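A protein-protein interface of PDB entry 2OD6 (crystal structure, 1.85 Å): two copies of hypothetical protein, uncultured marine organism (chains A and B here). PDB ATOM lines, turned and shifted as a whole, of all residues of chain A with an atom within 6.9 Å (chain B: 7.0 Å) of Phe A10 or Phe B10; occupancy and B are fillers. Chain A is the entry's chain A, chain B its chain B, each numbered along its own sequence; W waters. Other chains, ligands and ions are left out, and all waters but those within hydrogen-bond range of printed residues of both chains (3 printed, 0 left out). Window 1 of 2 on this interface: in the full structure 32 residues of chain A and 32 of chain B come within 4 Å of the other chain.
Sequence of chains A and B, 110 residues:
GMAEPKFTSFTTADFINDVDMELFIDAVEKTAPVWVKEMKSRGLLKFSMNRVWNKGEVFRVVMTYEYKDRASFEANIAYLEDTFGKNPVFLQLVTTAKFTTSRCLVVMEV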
ATOM      1  N   THR A   8      18.076   8.075   1.442  1.00  0.00           N
ATOM      2  CA  THR A   8      17.982   8.711   0.117  1.00  0.00           C
ATOM      3  C   THR A   8      16.850   8.140  -0.679  1.00  0.00           C
ATOM      4  O   THR A   8      16.710   6.935  -0.766  1.00  0.00           O
ATOM      5  CB  THR A   8      19.264   8.542  -0.702  1.00  0.00           C
ATOM      6  OG1 THR A   8      20.353   9.147   0.004  1.00  0.00           O
ATOM      7  CG2 THR A   8      19.181   9.263  -2.074  1.00  0.00           C
ATOM      8  N   SER A   9      16.040   9.031  -1.239  1.00  0.00           N
ATOM      9  CA  SER A   9      14.924   8.661  -2.087  1.00  0.00           C
ATOM     10  C   SER A   9      15.232   9.126  -3.505  1.00  0.00           C
ATOM     11  O   SER A   9      15.830  10.200  -3.673  1.00  0.00           O
ATOM     12  CB  SER A   9      13.682   9.317  -1.583  1.00  0.00           C
ATOM     13  OG  SER A   9      13.369   8.879  -0.292  1.00  0.00           O
ATOM     14  N   PHE A  10      14.842   8.318  -4.493  1.00  0.00           N
ATOM     15  CA  PHE A  10      14.999   8.647  -5.906  1.00  0.00           C
ATOM     16  C   PHE A  10      13.666   8.591  -6.502  1.00  0.00           C
ATOM     17  O   PHE A  10      13.074   7.522  -6.537  1.00  0.00           O
ATOM     18  CB  PHE A  10      15.884   7.628  -6.632  1.00  0.00           C
ATOM     19  CG  PHE A  10      17.221   7.443  -6.006  1.00  0.00           C
ATOM     20  CD1 PHE A  10      18.276   8.285  -6.307  1.00  0.00           C
ATOM     21  CD2 PHE A  10      17.420   6.439  -5.082  1.00  0.00           C
ATOM     22  CE1 PHE A  10      19.515   8.110  -5.712  1.00  0.00           C
ATOM     23  CE2 PHE A  10      18.660   6.261  -4.485  1.00  0.00           C
ATOM     24  CZ  PHE A  10      19.705   7.098  -4.789  1.00  0.00           C
ATOM     25  N   THR A  11      13.141   9.737  -6.887  1.00  0.00           N
ATOM     26  CA  THR A  11      11.803   9.739  -7.539  1.00  0.00           C
ATOM     27  C   THR A  11      12.045   9.880  -9.018  1.00  0.00           C
ATOM     28  O   THR A  11      12.715  10.859  -9.451  1.00  0.00           O
ATOM     29  CB  THR A  11      10.996  10.910  -6.978  1.00  0.00           C
ATOM     30  OG1 THR A  11      10.804  10.713  -5.572  1.00  0.00           O
ATOM     31  CG2 THR A  11       9.652  11.053  -7.653  1.00  0.00           C
ATOM     32  N   THR A  12      11.411   9.009  -9.802  1.00  0.00           N
ATOM     33  CA  THR A  12      11.461   9.091 -11.246  1.00  0.00           C
ATOM     34  C   THR A  12      10.118   9.605 -11.683  1.00  0.00           C
ATOM     35  O   THR A  12       9.054   9.080 -11.281  1.00  0.00           O
ATOM     36  CB  THR A  12      11.822   7.730 -11.951  1.00  0.00           C
ATOM     37  OG1 THR A  12      13.126   7.319 -11.508  1.00  0.00           O
ATOM     38  CG2 THR A  12      11.807   7.882 -13.487  1.00  0.00           C
ATOM     39  N   SER A  48      18.453  17.127  -5.971  1.00  0.00           N
ATOM     40  CA  SER A  48      18.897  17.282  -7.386  1.00  0.00           C
ATOM     41  C   SER A  48      17.846  16.798  -8.289  1.00  0.00           C
ATOM     42  O   SER A  48      17.090  15.947  -7.876  1.00  0.00           O
ATOM     43  CB  SER A  48      20.263  16.622  -7.670  1.00  0.00           C
ATOM     44  OG  SER A  48      20.211  15.207  -7.718  1.00  0.00           O
ATOM     45  N   ASN A  50      17.498  15.528 -12.451  1.00  0.00           N
ATOM     46  CA  ASN A  50      18.476  14.985 -13.430  1.00  0.00           C
ATOM     47  C   ASN A  50      17.736  14.542 -14.602  1.00  0.00           C
ATOM     48  O   ASN A  50      16.799  13.818 -14.387  1.00  0.00           O
ATOM     49  CB  ASN A  50      19.221  13.796 -12.793  1.00  0.00           C
ATOM     50  CG  ASN A  50      19.898  14.155 -11.485  1.00  0.00           C
ATOM     51  OD1 ASN A  50      21.039  14.612 -11.491  1.00  0.00           O
ATOM     52  ND2 ASN A  50      19.193  13.918 -10.314  1.00  0.00           N
ATOM     53  N   VAL A  52      17.143  12.341 -17.806  1.00  0.00           N
ATOM     54  CA  VAL A  52      17.654  11.040 -18.248  1.00  0.00           C
ATOM     55  C   VAL A  52      17.743  11.102 -19.780  1.00  0.00           C
ATOM     56  O   VAL A  52      16.728  11.342 -20.450  1.00  0.00           O
ATOM     57  CB  VAL A  52      16.771   9.856 -17.794  1.00  0.00           C
ATOM     58  CG1 VAL A  52      17.319   8.486 -18.442  1.00  0.00           C
ATOM     59  CG2 VAL A  52      16.694   9.748 -16.197  1.00  0.00           C
ATOM     60  N   LYS A  55      17.562   6.720 -22.455  1.00  0.00           N
ATOM     61  CA  LYS A  55      16.407   5.814 -22.542  1.00  0.00           C
ATOM     62  C   LYS A  55      15.602   6.106 -23.750  1.00  0.00           C
ATOM     63  O   LYS A  55      14.410   5.710 -23.858  1.00  0.00           O
ATOM     64  CB  LYS A  55      15.548   5.945 -21.278  1.00  0.00           C
ATOM     65  CG  LYS A  55      16.254   5.538 -20.067  1.00  0.00           C
ATOM     66  CD  LYS A  55      16.677   4.119 -20.115  1.00  0.00           C
ATOM     67  CE  LYS A  55      17.445   3.794 -18.828  1.00  0.00           C
ATOM     68  NZ  LYS A  55      18.046   2.438 -18.843  1.00  0.00           N
ATOM     69  N   VAL A  62      15.111  12.227 -12.850  1.00  0.00           N
ATOM     70  CA  VAL A  62      15.225  11.604 -11.562  1.00  0.00           C
ATOM     71  C   VAL A  62      15.555  12.696 -10.545  1.00  0.00           C
ATOM     72  O   VAL A  62      16.508  13.449 -10.706  1.00  0.00           O
ATOM     73  CB  VAL A  62      16.335  10.484 -11.526  1.00  0.00           C
ATOM     74  CG1 VAL A  62      16.547   9.924 -10.084  1.00  0.00           C
ATOM     75  CG2 VAL A  62      15.946   9.358 -12.481  1.00  0.00           C
ATOM     76  N   MET A  63      14.764  12.724  -9.475  1.00  0.00           N
ATOM     77  CA  MET A  63      14.929  13.618  -8.365  1.00  0.00           C
ATOM     78  C   MET A  63      15.538  12.894  -7.150  1.00  0.00           C
ATOM     79  O   MET A  63      15.060  11.816  -6.731  1.00  0.00           O
ATOM     80  CB  MET A  63      13.567  14.221  -8.070  1.00  0.00           C
ATOM     81  CG  MET A  63      13.090  15.096  -9.230  1.00  0.00           C
ATOM     82  SD  MET A  63      11.425  15.954  -8.681  1.00  0.00           S
ATOM     83  CE  MET A  63      10.242  14.502  -8.753  1.00  0.00           C
ATOM     84  N   THR A  64      16.603  13.425  -6.580  1.00  0.00           N
ATOM     85  CA  THR A  64      17.191  12.757  -5.491  1.00  0.00           C
ATOM     86  C   THR A  64      16.996  13.641  -4.255  1.00  0.00           C
ATOM     87  O   THR A  64      17.190  14.841  -4.326  1.00  0.00           O
ATOM     88  CB  THR A  64      18.700  12.465  -5.719  1.00  0.00           C
ATOM     89  OG1 THR A  64      19.399  13.701  -5.646  1.00  0.00           O
ATOM     90  CG2 THR A  64      18.947  11.804  -7.081  1.00  0.00           C
ATOM     91  N   TYR A  65      16.583  13.026  -3.143  1.00  0.00           N
ATOM     92  CA  TYR A  65      16.464  13.678  -1.849  1.00  0.00           C
ATOM     93  C   TYR A  65      17.434  13.012  -0.887  1.00  0.00           C
ATOM     94  O   TYR A  65      17.289  11.836  -0.587  1.00  0.00           O
ATOM     95  CB  TYR A  65      15.049  13.486  -1.344  1.00  0.00           C
ATOM     96  CG  TYR A  65      14.039  14.090  -2.221  1.00  0.00           C
ATOM     97  CD1 TYR A  65      13.533  13.359  -3.295  1.00  0.00           C
ATOM     98  CD2 TYR A  65      13.586  15.390  -2.030  1.00  0.00           C
ATOM     99  CE1 TYR A  65      12.566  13.894  -4.170  1.00  0.00           C
ATOM    100  CE2 TYR A  65      12.594  15.942  -2.915  1.00  0.00           C
ATOM    101  CZ  TYR A  65      12.120  15.177  -3.958  1.00  0.00           C
ATOM    102  OH  TYR A  65      11.200  15.706  -4.789  1.00  0.00           O
ATOM    103  N   GLU A  66      18.441  13.717  -0.427  1.00  0.00           N
ATOM    104  CA  GLU A  66      19.405  13.130   0.452  1.00  0.00           C
ATOM    105  C   GLU A  66      19.126  13.627   1.877  1.00  0.00           C
ATOM    106  O   GLU A  66      19.317  14.795   2.162  1.00  0.00           O
ATOM    107  CB  GLU A  66      20.823  13.547   0.056  1.00  0.00           C
ATOM    108  CG  GLU A  66      21.347  12.793  -1.151  1.00  0.00           C
ATOM    109  CD  GLU A  66      22.611  13.361  -1.704  1.00  0.00           C
ATOM    110  OE1 GLU A  66      23.613  13.548  -0.963  1.00  0.00           O
ATOM    111  OE2 GLU A  66      22.593  13.602  -2.920  1.00  0.00           O
ATOM    112  N   THR A 100       7.533   7.369  -9.643  1.00  0.00           N
ATOM    113  CA  THR A 100       7.822   6.156  -8.875  1.00  0.00           C
ATOM    114  C   THR A 100       9.048   6.455  -8.034  1.00  0.00           C
ATOM    115  O   THR A 100      10.000   7.052  -8.527  1.00  0.00           O
ATOM    116  CB  THR A 100       8.035   4.890  -9.784  1.00  0.00           C
ATOM    117  OG1 THR A 100       9.015   5.166 -10.799  1.00  0.00           O
ATOM    118  CG2 THR A 100       6.718   4.447 -10.441  1.00  0.00           C
ATOM    119  N   THR A 101       9.004   6.096  -6.749  1.00  0.00           N
ATOM    120  CA  THR A 101      10.104   6.404  -5.825  1.00  0.00           C
ATOM    121  C   THR A 101      10.771   5.163  -5.274  1.00  0.00           C
ATOM    122  O   THR A 101      10.107   4.227  -4.859  1.00  0.00           O
ATOM    123  CB  THR A 101       9.662   7.303  -4.666  1.00  0.00           C
ATOM    124  OG1 THR A 101       9.092   8.493  -5.203  1.00  0.00           O
ATOM    125  CG2 THR A 101      10.874   7.712  -3.801  1.00  0.00           C
ATOM    126  N   SER A 102      12.100   5.173  -5.272  1.00  0.00           N
ATOM    127  CA  SER A 102      12.846   4.147  -4.613  1.00  0.00           C
ATOM    128  C   SER A 102      13.465   4.782  -3.402  1.00  0.00           C
ATOM    129  O   SER A 102      14.351   5.628  -3.516  1.00  0.00           O
ATOM    130  CB  SER A 102      13.855   3.500  -5.568  1.00  0.00           C
ATOM    131  OG  SER A 102      13.104   2.620  -6.412  1.00  0.00           O
ATOM    132  N   ARG A 103      12.997   4.366  -2.231  1.00  0.00           N
ATOM    133  CA  ARG A 103      13.518   4.864  -0.957  1.00  0.00           C
ATOM    134  C   ARG A 103      14.563   3.893  -0.416  1.00  0.00           C
ATOM    135  O   ARG A 103      14.308   2.676  -0.333  1.00  0.00           O
ATOM    136  CB  ARG A 103      12.379   5.049   0.038  1.00  0.00           C
ATOM    137  CG  ARG A 103      11.266   5.959  -0.489  1.00  0.00           C
ATOM    138  CD  ARG A 103      10.216   6.265   0.559  1.00  0.00           C
ATOM    139  NE  ARG A 103       9.498   7.496   0.231  1.00  0.00           N
ATOM    140  CZ  ARG A 103       8.440   7.572  -0.572  1.00  0.00           C
ATOM    141  NH1 ARG A 103       7.917   6.484  -1.129  1.00  0.00           N
ATOM    142  NH2 ARG A 103       7.882   8.756  -0.803  1.00  0.00           N
ATOM    143  N   CYS A 104      15.709   4.457  -0.021  1.00  0.00           N
ATOM    144  CA  CYS A 104      16.925   3.709   0.322  1.00  0.00           C
ATOM    145  C   CYS A 104      17.557   4.140   1.635  1.00  0.00           C
ATOM    146  O   CYS A 104      17.274   5.205   2.141  1.00  0.00           O
ATOM    147  CB  CYS A 104      17.986   3.907  -0.785  1.00  0.00           C
ATOM    148  SG  CYS A 104      17.323   3.467  -2.430  1.00  0.00           S
ATOM    149  N   THR B   8      25.386  12.670 -14.013  1.00  0.00           N
ATOM    150  CA  THR B   8      25.187  11.707 -12.954  1.00  0.00           C
ATOM    151  C   THR B   8      24.519  10.464 -13.549  1.00  0.00           C
ATOM    152  O   THR B   8      23.669  10.585 -14.407  1.00  0.00           O
ATOM    153  CB  THR B   8      24.346  12.295 -11.780  1.00  0.00           C
ATOM    154  OG1 THR B   8      24.982  13.475 -11.241  1.00  0.00           O
ATOM    155  CG2 THR B   8      24.114  11.227 -10.673  1.00  0.00           C
ATOM    156  N   SER B   9      24.994   9.299 -13.139  1.00  0.00           N
ATOM    157  CA  SER B   9      24.458   7.990 -13.511  1.00  0.00           C
ATOM    158  C   SER B   9      23.887   7.274 -12.297  1.00  0.00           C
ATOM    159  O   SER B   9      24.460   7.323 -11.220  1.00  0.00           O
ATOM    160  CB  SER B   9      25.562   7.117 -14.106  1.00  0.00           C
ATOM    161  OG  SER B   9      26.104   7.746 -15.234  1.00  0.00           O
ATOM    162  N   PHE B  10      22.751   6.607 -12.510  1.00  0.00           N
ATOM    163  CA  PHE B  10      22.054   5.816 -11.509  1.00  0.00           C
ATOM    164  C   PHE B  10      21.981   4.403 -12.068  1.00  0.00           C
ATOM    165  O   PHE B  10      21.378   4.187 -13.091  1.00  0.00           O
ATOM    166  CB  PHE B  10      20.627   6.363 -11.245  1.00  0.00           C
ATOM    167  CG  PHE B  10      20.606   7.803 -10.795  1.00  0.00           C
ATOM    168  CD1 PHE B  10      20.882   8.132  -9.490  1.00  0.00           C
ATOM    169  CD2 PHE B  10      20.306   8.827 -11.692  1.00  0.00           C
ATOM    170  CE1 PHE B  10      20.878   9.464  -9.081  1.00  0.00           C
ATOM    171  CE2 PHE B  10      20.288  10.159 -11.277  1.00  0.00           C
ATOM    172  CZ  PHE B  10      20.590  10.464  -9.978  1.00  0.00           C
ATOM    173  N   THR B  11      22.695   3.487 -11.425  1.00  0.00           N
ATOM    174  CA  THR B  11      22.656   2.074 -11.732  1.00  0.00           C
ATOM    175  C   THR B  11      21.945   1.307 -10.639  1.00  0.00           C
ATOM    176  O   THR B  11      22.373   1.292  -9.468  1.00  0.00           O
ATOM    177  CB  THR B  11      24.079   1.473 -11.860  1.00  0.00           C
ATOM    178  OG1 THR B  11      24.808   2.171 -12.864  1.00  0.00           O
ATOM    179  CG2 THR B  11      24.023  -0.039 -12.162  1.00  0.00           C
ATOM    180  N   THR B  12      20.857   0.667 -11.046  1.00  0.00           N
ATOM    181  CA  THR B  12      20.080  -0.217 -10.221  1.00  0.00           C
ATOM    182  C   THR B  12      20.533  -1.668 -10.485  1.00  0.00           C
ATOM    183  O   THR B  12      20.581  -2.112 -11.644  1.00  0.00           O
ATOM    184  CB  THR B  12      18.579  -0.029 -10.535  1.00  0.00           C
ATOM    185  OG1 THR B  12      18.194   1.333 -10.253  1.00  0.00           O
ATOM    186  CG2 THR B  12      17.694  -1.014  -9.731  1.00  0.00           C
ATOM    187  N   SER B  48      27.814   6.633  -4.344  1.00  0.00           N
ATOM    188  CA  SER B  48      27.098   6.044  -3.243  1.00  0.00           C
ATOM    189  C   SER B  48      26.393   4.768  -3.667  1.00  0.00           C
ATOM    190  O   SER B  48      26.074   4.576  -4.840  1.00  0.00           O
ATOM    191  CB  SER B  48      26.106   7.035  -2.619  1.00  0.00           C
ATOM    192  OG  SER B  48      24.971   7.281  -3.435  1.00  0.00           O
ATOM    193  N   ASN B  50      23.145   2.330  -2.279  1.00  0.00           N
ATOM    194  CA  ASN B  50      21.944   2.631  -1.533  1.00  0.00           C
ATOM    195  C   ASN B  50      21.007   1.439  -1.607  1.00  0.00           C
ATOM    196  O   ASN B  50      20.668   1.007  -2.690  1.00  0.00           O
ATOM    197  CB  ASN B  50      21.258   3.841  -2.164  1.00  0.00           C
ATOM    198  CG  ASN B  50      22.142   5.071  -2.217  1.00  0.00           C
ATOM    199  OD1 ASN B  50      22.189   5.830  -1.253  1.00  0.00           O
ATOM    200  ND2 ASN B  50      22.803   5.304  -3.363  1.00  0.00           N
ATOM    201  N   ARG B  51      20.603   0.920  -0.462  1.00  0.00           N
ATOM    202  CA  ARG B  51      19.821  -0.308  -0.423  1.00  0.00           C
ATOM    203  C   ARG B  51      18.338   0.045  -0.415  1.00  0.00           C
ATOM    204  O   ARG B  51      17.904   0.832   0.414  1.00  0.00           O
ATOM    205  CB  ARG B  51      20.217  -1.140   0.801  1.00  0.00           C
ATOM    206  CG  ARG B  51      19.289  -2.307   1.115  1.00  0.00           C
ATOM    207  CD  ARG B  51      19.495  -3.524   0.224  1.00  0.00           C
ATOM    208  NE  ARG B  51      18.422  -4.515   0.469  1.00  0.00           N
ATOM    209  CZ  ARG B  51      18.466  -5.482   1.394  1.00  0.00           C
ATOM    210  NH1 ARG B  51      19.516  -5.645   2.198  1.00  0.00           N
ATOM    211  NH2 ARG B  51      17.438  -6.312   1.519  1.00  0.00           N
ATOM    212  N   VAL B  52      17.582  -0.529  -1.345  1.00  0.00           N
ATOM    213  CA  VAL B  52      16.179  -0.165  -1.559  1.00  0.00           C
ATOM    214  C   VAL B  52      15.332  -0.851  -0.488  1.00  0.00           C
ATOM    215  O   VAL B  52      15.451  -2.051  -0.319  1.00  0.00           O
ATOM    216  CB  VAL B  52      15.699  -0.554  -2.985  1.00  0.00           C
ATOM    217  CG1 VAL B  52      14.205  -0.247  -3.179  1.00  0.00           C
ATOM    218  CG2 VAL B  52      16.509   0.203  -4.033  1.00  0.00           C
ATOM    219  N   VAL B  62      20.697   0.845  -5.481  1.00  0.00           N
ATOM    220  CA  VAL B  62      20.896   1.898  -6.467  1.00  0.00           C
ATOM    221  C   VAL B  62      22.252   2.477  -6.182  1.00  0.00           C
ATOM    222  O   VAL B  62      22.506   2.895  -5.061  1.00  0.00           O
ATOM    223  CB  VAL B  62      19.817   2.988  -6.392  1.00  0.00           C
ATOM    224  CG1 VAL B  62      20.165   4.214  -7.352  1.00  0.00           C
ATOM    225  CG2 VAL B  62      18.423   2.391  -6.686  1.00  0.00           C
ATOM    226  N   MET B  63      23.129   2.475  -7.184  1.00  0.00           N
ATOM    227  CA  MET B  63      24.440   3.102  -7.109  1.00  0.00           C
ATOM    228  C   MET B  63      24.434   4.403  -7.886  1.00  0.00           C
ATOM    229  O   MET B  63      23.895   4.468  -9.007  1.00  0.00           O
ATOM    230  CB  MET B  63      25.545   2.191  -7.659  1.00  0.00           C
ATOM    231  CG  MET B  63      25.913   1.056  -6.713  1.00  0.00           C
ATOM    232  SD  MET B  63      26.927  -0.378  -7.582  1.00  0.00           S
ATOM    233  CE  MET B  63      25.643  -0.828  -8.911  1.00  0.00           C
ATOM    234  N   THR B  64      25.041   5.429  -7.284  1.00  0.00           N
ATOM    235  CA  THR B  64      25.072   6.748  -7.885  1.00  0.00           C
ATOM    236  C   THR B  64      26.489   7.164  -8.177  1.00  0.00           C
ATOM    237  O   THR B  64      27.360   7.061  -7.309  1.00  0.00           O
ATOM    238  CB  THR B  64      24.403   7.829  -7.018  1.00  0.00           C
ATOM    239  OG1 THR B  64      25.182   8.040  -5.851  1.00  0.00           O
ATOM    240  CG2 THR B  64      23.048   7.402  -6.602  1.00  0.00           C
ATOM    241  N   TYR B  65      26.701   7.604  -9.414  1.00  0.00           N
ATOM    242  CA  TYR B  65      27.992   8.150  -9.877  1.00  0.00           C
ATOM    243  C   TYR B  65      27.803   9.581 -10.309  1.00  0.00           C
ATOM    244  O   TYR B  65      27.083   9.863 -11.251  1.00  0.00           O
ATOM    245  CB  TYR B  65      28.604   7.334 -11.011  1.00  0.00           C
ATOM    246  CG  TYR B  65      28.712   5.841 -10.761  1.00  0.00           C
ATOM    247  CD1 TYR B  65      27.614   5.015 -10.951  1.00  0.00           C
ATOM    248  CD2 TYR B  65      29.907   5.255 -10.383  1.00  0.00           C
ATOM    249  CE1 TYR B  65      27.676   3.672 -10.732  1.00  0.00           C
ATOM    250  CE2 TYR B  65      29.995   3.883 -10.182  1.00  0.00           C
ATOM    251  CZ  TYR B  65      28.857   3.098 -10.351  1.00  0.00           C
ATOM    252  OH  TYR B  65      28.887   1.741 -10.175  1.00  0.00           O
ATOM    253  N   GLU B  66      28.470  10.481  -9.596  1.00  0.00           N
ATOM    254  CA  GLU B  66      28.414  11.916  -9.840  1.00  0.00           C
ATOM    255  C   GLU B  66      29.734  12.377 -10.428  1.00  0.00           C
ATOM    256  O   GLU B  66      30.749  12.289  -9.774  1.00  0.00           O
ATOM    257  CB  GLU B  66      28.172  12.644  -8.544  1.00  0.00           C
ATOM    258  CG  GLU B  66      26.750  12.445  -8.036  1.00  0.00           C
ATOM    259  CD  GLU B  66      26.503  13.095  -6.690  1.00  0.00           C
ATOM    260  OE1 GLU B  66      26.845  14.287  -6.546  1.00  0.00           O
ATOM    261  OE2 GLU B  66      25.957  12.414  -5.802  1.00  0.00           O
ATOM    262  N   THR B 100      20.719  -1.998 -14.586  1.00  0.00           N
ATOM    263  CA  THR B 100      20.073  -1.055 -15.495  1.00  0.00           C
ATOM    264  C   THR B 100      20.487   0.328 -15.083  1.00  0.00           C
ATOM    265  O   THR B 100      20.321   0.676 -13.918  1.00  0.00           O
ATOM    266  CB  THR B 100      18.539  -1.190 -15.468  1.00  0.00           C
ATOM    267  OG1 THR B 100      17.968  -0.297 -16.432  1.00  0.00           O
ATOM    268  CG2 THR B 100      17.953  -0.898 -14.072  1.00  0.00           C
ATOM    269  N   THR B 101      21.049   1.095 -16.023  1.00  0.00           N
ATOM    270  CA  THR B 101      21.618   2.415 -15.742  1.00  0.00           C
ATOM    271  C   THR B 101      20.874   3.535 -16.472  1.00  0.00           C
ATOM    272  O   THR B 101      20.451   3.383 -17.633  1.00  0.00           O
ATOM    273  CB  THR B 101      23.137   2.496 -16.083  1.00  0.00           C
ATOM    274  OG1 THR B 101      23.838   1.506 -15.340  1.00  0.00           O
ATOM    275  CG2 THR B 101      23.717   3.862 -15.721  1.00  0.00           C
ATOM    276  N   SER B 102      20.672   4.617 -15.732  1.00  0.00           N
ATOM    277  CA  SER B 102      20.116   5.863 -16.220  1.00  0.00           C
ATOM    278  C   SER B 102      21.207   6.917 -16.141  1.00  0.00           C
ATOM    279  O   SER B 102      21.702   7.224 -15.057  1.00  0.00           O
ATOM    280  CB  SER B 102      18.905   6.281 -15.399  1.00  0.00           C
ATOM    281  OG  SER B 102      17.797   5.476 -15.763  1.00  0.00           O
ATOM    282  N   ARG B 103      21.578   7.423 -17.323  1.00  0.00           N
ATOM    283  CA  ARG B 103      22.597   8.459 -17.479  1.00  0.00           C
ATOM    284  C   ARG B 103      21.923   9.799 -17.666  1.00  0.00           C
ATOM    285  O   ARG B 103      21.022   9.926 -18.480  1.00  0.00           O
ATOM    286  CB  ARG B 103      23.497   8.108 -18.671  1.00  0.00           C
ATOM    287  CG  ARG B 103      24.162   6.809 -18.428  1.00  0.00           C
ATOM    288  CD  ARG B 103      25.183   6.387 -19.418  1.00  0.00           C
ATOM    289  NE  ARG B 103      25.781   5.166 -18.878  1.00  0.00           N
ATOM    290  CZ  ARG B 103      26.605   4.346 -19.513  1.00  0.00           C
ATOM    291  NH1 ARG B 103      26.999   4.586 -20.763  1.00  0.00           N
ATOM    292  NH2 ARG B 103      27.045   3.266 -18.875  1.00  0.00           N
ATOM    293  N   CYS B 104      22.384  10.794 -16.909  1.00  0.00           N
ATOM    294  CA  CYS B 104      21.671  12.013 -16.699  1.00  0.00           C
ATOM    295  C   CYS B 104      22.535  13.250 -16.822  1.00  0.00           C
ATOM    296  O   CYS B 104      23.736  13.228 -16.566  1.00  0.00           O
ATOM    297  CB  CYS B 104      20.987  12.015 -15.317  1.00  0.00           C
ATOM    298  SG  CYS B 104      19.887  10.637 -15.058  1.00  0.00           S
HETATM  299  O   HOH W   1      25.358  14.065  -3.596  1.00  0.00           O
HETATM  300  O   HOH W   2      23.038  14.558  -9.488  1.00  0.00           O
HETATM  301  O   HOH W   3      22.884   8.532  -1.325  1.00  0.00           O
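NZ of Lys A55 is in hydrogen-bond range of O of Thr B101 (2.9 Å).
Phe A10 touches just these residues of chain B: Phe B10, Asn B50, Val B62 and Thr B64.
Printed residues of chain B within 4 Å of Arg A103: Val B52 (3.6 Å).
Of the printed residues of chain B, Cys A104 touches Asn B50, Arg B51 and Val B52.
Of the printed residues of chain A, Arg B51 touches Cys A104.
Of the printed residues of chain A, Val B52 touches Arg A103 and Cys A104.
Met B63 touches none of the printed residues of chain A.
Of the printed residues of chain A, Thr B101 touches Lys A55 (2.9 Å).
The nearest residue of chain A that does not touch Phe B10 is Ser A48 (5.3 Å).
The nearest printed residue of chain A that does not touch Asn B50 is Arg A103 (6.9 Å).
Hydrophobic or aromatic side chains of chain A that line the printed part of chain B: Phe A10, Val A52 and Val A62.
Hydrophobic or aromatic side chains of chain B within 4 Å of the printed part of chain A: Phe B10, Val B52 and Val B62.
Among the printed residues, no Asp or Glu carboxylate lies within 4 Å of a Lys or Arg side-chain nitrogen of the other chain.
The backbone carbonyl oxygen (O) of Thr A8 lies within hydrogen-bond range of the backbone NH (N) of Cys A104 (2.8 Å).
The side-chain hydroxyl of Ser A48 lies within hydrogen-bond range of the side-chain amide nitrogen of Asn A50, 3.1 Å away.
ND2 of Asn A50 lies within hydrogen-bond range of O of Val A62 (2.8 Å).
O of Phe B10 lies within hydrogen-bond range of N of Ser B102, at 2.8 Å.
The side-chain hydroxyl of Ser B48 lies within hydrogen-bond range of the side-chain amide nitrogen of Asn B50.
The side-chain hydroxyl of Ser B48 lies within hydrogen-bond range of the side-chain hydroxyl of Thr B64 (2.5 Å).
Thr A8 touches Asn B50, but with the chains exchanged Asn A50 does not touch Thr B8 (4.05 Å).
Phe A10 touches Val B62, and with the chains exchanged Val A62 touches Phe B10.
Val A52 touches Arg B103, and with the chains exchanged Arg A103 touches Val B52.
Val A52 touches Cys B104, and with the chains exchanged Cys A104 touches Val B52.
Positions printed for both chains: 8, 9, 10, 11, 12, 48, 50, 52, 62, 63, 64, 65, 66, 100, 101, 102, 103 and 104.
Of the 18 pairs that touch across the chains among the printed residues, 13 have their exchanged pair printed and touching as well.
Water W3 lies within hydrogen-bond range of OD1 of Asn B50 (2.8 Å), OG1 of Thr A8 (2.9 Å) and OG of Ser B48 (3.2 Å).
Water W1 lies within hydrogen-bond range of OE2 of Glu B66 and OE2 of Glu A66.
Water W2 lies within hydrogen-bond range of the side-chain amide oxygen (OD1) of Asn A50 (2.8 Å), the side-chain hydroxyl (OG1) of Thr B8 (2.8 Å) and the side-chain hydroxyl (OG) of Ser A48 (3.4 Å).
Among the printed residues, merely in contact across the chains: Cys A104 with Arg B51, Val A52 with Cys B104, Lys A55 with Ser B102, Cys A104 with Asn B50, Val A52 with Arg B103, Asn A50 with Cys B104, Thr A64 with Phe B10, Arg A103 with Val B52, Lys A55 with Thr B100, Phe A10 with Thr B64, Cys A104 with Val B52, Asn A50 with Phe B10, Phe A10 with Val B62, Phe A10 with Asn B50, Phe A10 with Phe B10, Val A62 with Phe B10 and Thr A8 with Asn B50.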
